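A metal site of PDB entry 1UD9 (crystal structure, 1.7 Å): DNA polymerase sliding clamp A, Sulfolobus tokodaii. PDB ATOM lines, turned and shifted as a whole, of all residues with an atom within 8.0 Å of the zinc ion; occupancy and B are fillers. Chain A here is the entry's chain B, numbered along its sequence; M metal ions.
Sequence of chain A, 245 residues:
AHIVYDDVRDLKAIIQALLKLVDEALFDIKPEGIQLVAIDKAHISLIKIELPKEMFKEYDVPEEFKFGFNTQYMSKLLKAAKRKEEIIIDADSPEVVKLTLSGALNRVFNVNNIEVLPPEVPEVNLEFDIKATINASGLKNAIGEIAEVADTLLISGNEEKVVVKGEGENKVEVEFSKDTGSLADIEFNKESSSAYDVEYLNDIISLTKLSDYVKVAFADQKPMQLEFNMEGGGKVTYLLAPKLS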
ATOM      1  N   ALA A 150     -23.258 -37.254  -5.259  1.00  0.00           N
ATOM      2  CA  ALA A 150     -23.578 -36.301  -6.322  1.00  0.00           C
ATOM      3  C   ALA A 150     -23.826 -34.896  -5.748  1.00  0.00           C
ATOM      4  O   ALA A 150     -24.057 -34.790  -4.547  1.00  0.00           O
ATOM      5  CB  ALA A 150     -24.829 -36.813  -7.062  1.00  0.00           C
ATOM      6  N   ASP A 151     -23.758 -33.840  -6.562  1.00  0.00           N
ATOM      7  CA  ASP A 151     -24.009 -32.494  -6.061  1.00  0.00           C
ATOM      8  C   ASP A 151     -25.463 -32.161  -6.324  1.00  0.00           C
ATOM      9  O   ASP A 151     -25.952 -31.165  -5.833  1.00  0.00           O
ATOM     10  CB  ASP A 151     -23.187 -31.371  -6.754  1.00  0.00           C
ATOM     11  CG  ASP A 151     -23.601 -29.896  -6.291  1.00  0.00           C
ATOM     12  OD1 ASP A 151     -23.839 -29.029  -7.160  1.00  0.00           O
ATOM     13  OD2 ASP A 151     -23.674 -29.576  -5.039  1.00  0.00           O
ATOM     14  N   THR A 152     -26.105 -33.004  -7.127  1.00  0.00           N
ATOM     15  CA  THR A 152     -27.480 -32.734  -7.558  1.00  0.00           C
ATOM     16  C   THR A 152     -28.447 -33.828  -7.372  1.00  0.00           C
ATOM     17  O   THR A 152     -28.157 -35.050  -7.554  1.00  0.00           O
ATOM     18  CB  THR A 152     -27.494 -32.370  -8.997  1.00  0.00           C
ATOM     19  OG1 THR A 152     -26.650 -31.255  -9.140  1.00  0.00           O
ATOM     20  CG2 THR A 152     -28.924 -32.009  -9.491  1.00  0.00           C
ATOM     21  N   TYR A 196     -32.336 -29.994  -8.076  1.00  0.00           N
ATOM     22  CA  TYR A 196     -31.988 -29.118  -6.953  1.00  0.00           C
ATOM     23  C   TYR A 196     -30.559 -29.436  -6.418  1.00  0.00           C
ATOM     24  O   TYR A 196     -30.069 -30.524  -6.560  1.00  0.00           O
ATOM     25  CB  TYR A 196     -33.011 -29.339  -5.824  1.00  0.00           C
ATOM     26  CG  TYR A 196     -34.453 -29.128  -6.220  1.00  0.00           C
ATOM     27  CD1 TYR A 196     -35.219 -30.208  -6.685  1.00  0.00           C
ATOM     28  CD2 TYR A 196     -35.011 -27.838  -6.328  1.00  0.00           C
ATOM     29  CE1 TYR A 196     -36.471 -29.976  -7.272  1.00  0.00           C
ATOM     30  CE2 TYR A 196     -36.248 -27.597  -6.891  1.00  0.00           C
ATOM     31  CZ  TYR A 196     -36.983 -28.709  -7.379  1.00  0.00           C
ATOM     32  OH  TYR A 196     -38.194 -28.472  -7.956  1.00  0.00           O
ATOM     33  N   ASP A 197     -29.931 -28.475  -5.709  1.00  0.00           N
ATOM     34  CA  ASP A 197     -28.594 -28.668  -5.133  1.00  0.00           C
ATOM     35  C   ASP A 197     -28.807 -29.485  -3.877  1.00  0.00           C
ATOM     36  O   ASP A 197     -29.437 -28.991  -2.933  1.00  0.00           O
ATOM     37  CB  ASP A 197     -28.019 -27.306  -4.720  1.00  0.00           C
ATOM     38  CG  ASP A 197     -26.634 -27.422  -4.141  1.00  0.00           C
ATOM     39  OD1 ASP A 197     -26.299 -28.407  -3.425  1.00  0.00           O
ATOM     40  OD2 ASP A 197     -25.899 -26.486  -4.375  1.00  0.00           O
ATOM     41  N   VAL A 198     -28.286 -30.695  -3.839  1.00  0.00           N
ATOM     42  CA  VAL A 198     -28.525 -31.596  -2.765  1.00  0.00           C
ATOM     43  C   VAL A 198     -27.813 -31.163  -1.488  1.00  0.00           C
ATOM     44  O   VAL A 198     -28.249 -31.576  -0.405  1.00  0.00           O
ATOM     45  CB  VAL A 198     -28.164 -33.047  -3.149  1.00  0.00           C
ATOM     46  CG1 VAL A 198     -26.633 -33.284  -3.164  1.00  0.00           C
ATOM     47  CG2 VAL A 198     -28.903 -34.028  -2.207  1.00  0.00           C
ATOM     48  N   GLU A 199     -26.796 -30.319  -1.624  1.00  0.00           N
ATOM     49  CA  GLU A 199     -26.066 -29.807  -0.433  1.00  0.00           C
ATOM     50  C   GLU A 199     -27.051 -29.003   0.419  1.00  0.00           C
ATOM     51  O   GLU A 199     -26.998 -29.067   1.655  1.00  0.00           O
ATOM     52  CB  GLU A 199     -24.965 -28.763  -0.752  1.00  0.00           C
ATOM     53  CG  GLU A 199     -23.937 -29.010  -1.835  1.00  0.00           C
ATOM     54  CD  GLU A 199     -23.052 -27.764  -2.100  1.00  0.00           C
ATOM     55  OE1 GLU A 199     -23.565 -26.711  -2.602  1.00  0.00           O
ATOM     56  OE2 GLU A 199     -21.832 -27.841  -1.797  1.00  0.00           O
ATOM     57  N   TYR A 200     -27.898 -28.215  -0.228  1.00  0.00           N
ATOM     58  CA  TYR A 200     -28.849 -27.422   0.551  1.00  0.00           C
ATOM     59  C   TYR A 200     -29.843 -28.318   1.257  1.00  0.00           C
ATOM     60  O   TYR A 200     -30.187 -28.111   2.442  1.00  0.00           O
ATOM     61  CB  TYR A 200     -29.612 -26.414  -0.320  1.00  0.00           C
ATOM     62  CG  TYR A 200     -28.784 -25.256  -0.755  1.00  0.00           C
ATOM     63  CD1 TYR A 200     -27.626 -25.446  -1.527  1.00  0.00           C
ATOM     64  CD2 TYR A 200     -29.145 -23.955  -0.383  1.00  0.00           C
ATOM     65  CE1 TYR A 200     -26.862 -24.352  -1.906  1.00  0.00           C
ATOM     66  CE2 TYR A 200     -28.374 -22.882  -0.750  1.00  0.00           C
ATOM     67  CZ  TYR A 200     -27.254 -23.083  -1.512  1.00  0.00           C
ATOM     68  OH  TYR A 200     -26.621 -21.972  -1.994  1.00  0.00           O
ATOM     69  N   LYS A 243     -32.551 -25.858 -10.032  1.00  0.00           N
ATOM     70  CA  LYS A 243     -31.476 -25.769 -11.006  1.00  0.00           C
ATOM     71  C   LYS A 243     -32.177 -26.123 -12.342  1.00  0.00           C
ATOM     72  O   LYS A 243     -33.349 -26.491 -12.361  1.00  0.00           O
ATOM     73  CB  LYS A 243     -30.396 -26.792 -10.769  1.00  0.00           C
ATOM     74  CG  LYS A 243     -29.596 -26.490  -9.482  1.00  0.00           C
ATOM     75  CD  LYS A 243     -29.028 -25.045  -9.544  1.00  0.00           C
ATOM     76  CE  LYS A 243     -27.894 -24.756  -8.506  1.00  0.00           C
ATOM     77  NZ  LYS A 243     -26.644 -25.659  -8.762  1.00  0.00           N
HETATM   78 ZN    ZN M   1     -24.098 -27.227  -4.999  1.00  0.00          ZN
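The side-chain carboxylate (OD2) of Asp 197 is bound to the zinc ion (2.0 Å).
The side-chain carboxylate (OD2) of Asp 151 is bound to the zinc ion, at 2.4 Å.
The zinc ion is bound by OE1 of Glu 199 (2.5 Å).
The zinc ion has three donor atoms within binding distance.
Slightly farther from the zinc ion lies the side-chain carboxylate (OD1) of Asp 151 (2.8 Å).
Of the 9 residues printed, 3 come within 4 Å of the zinc ion.
The backbone carbonyl oxygen of Asp 151 is in hydrogen-bond range of the backbone NH of Val 198 (3.1 Å).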
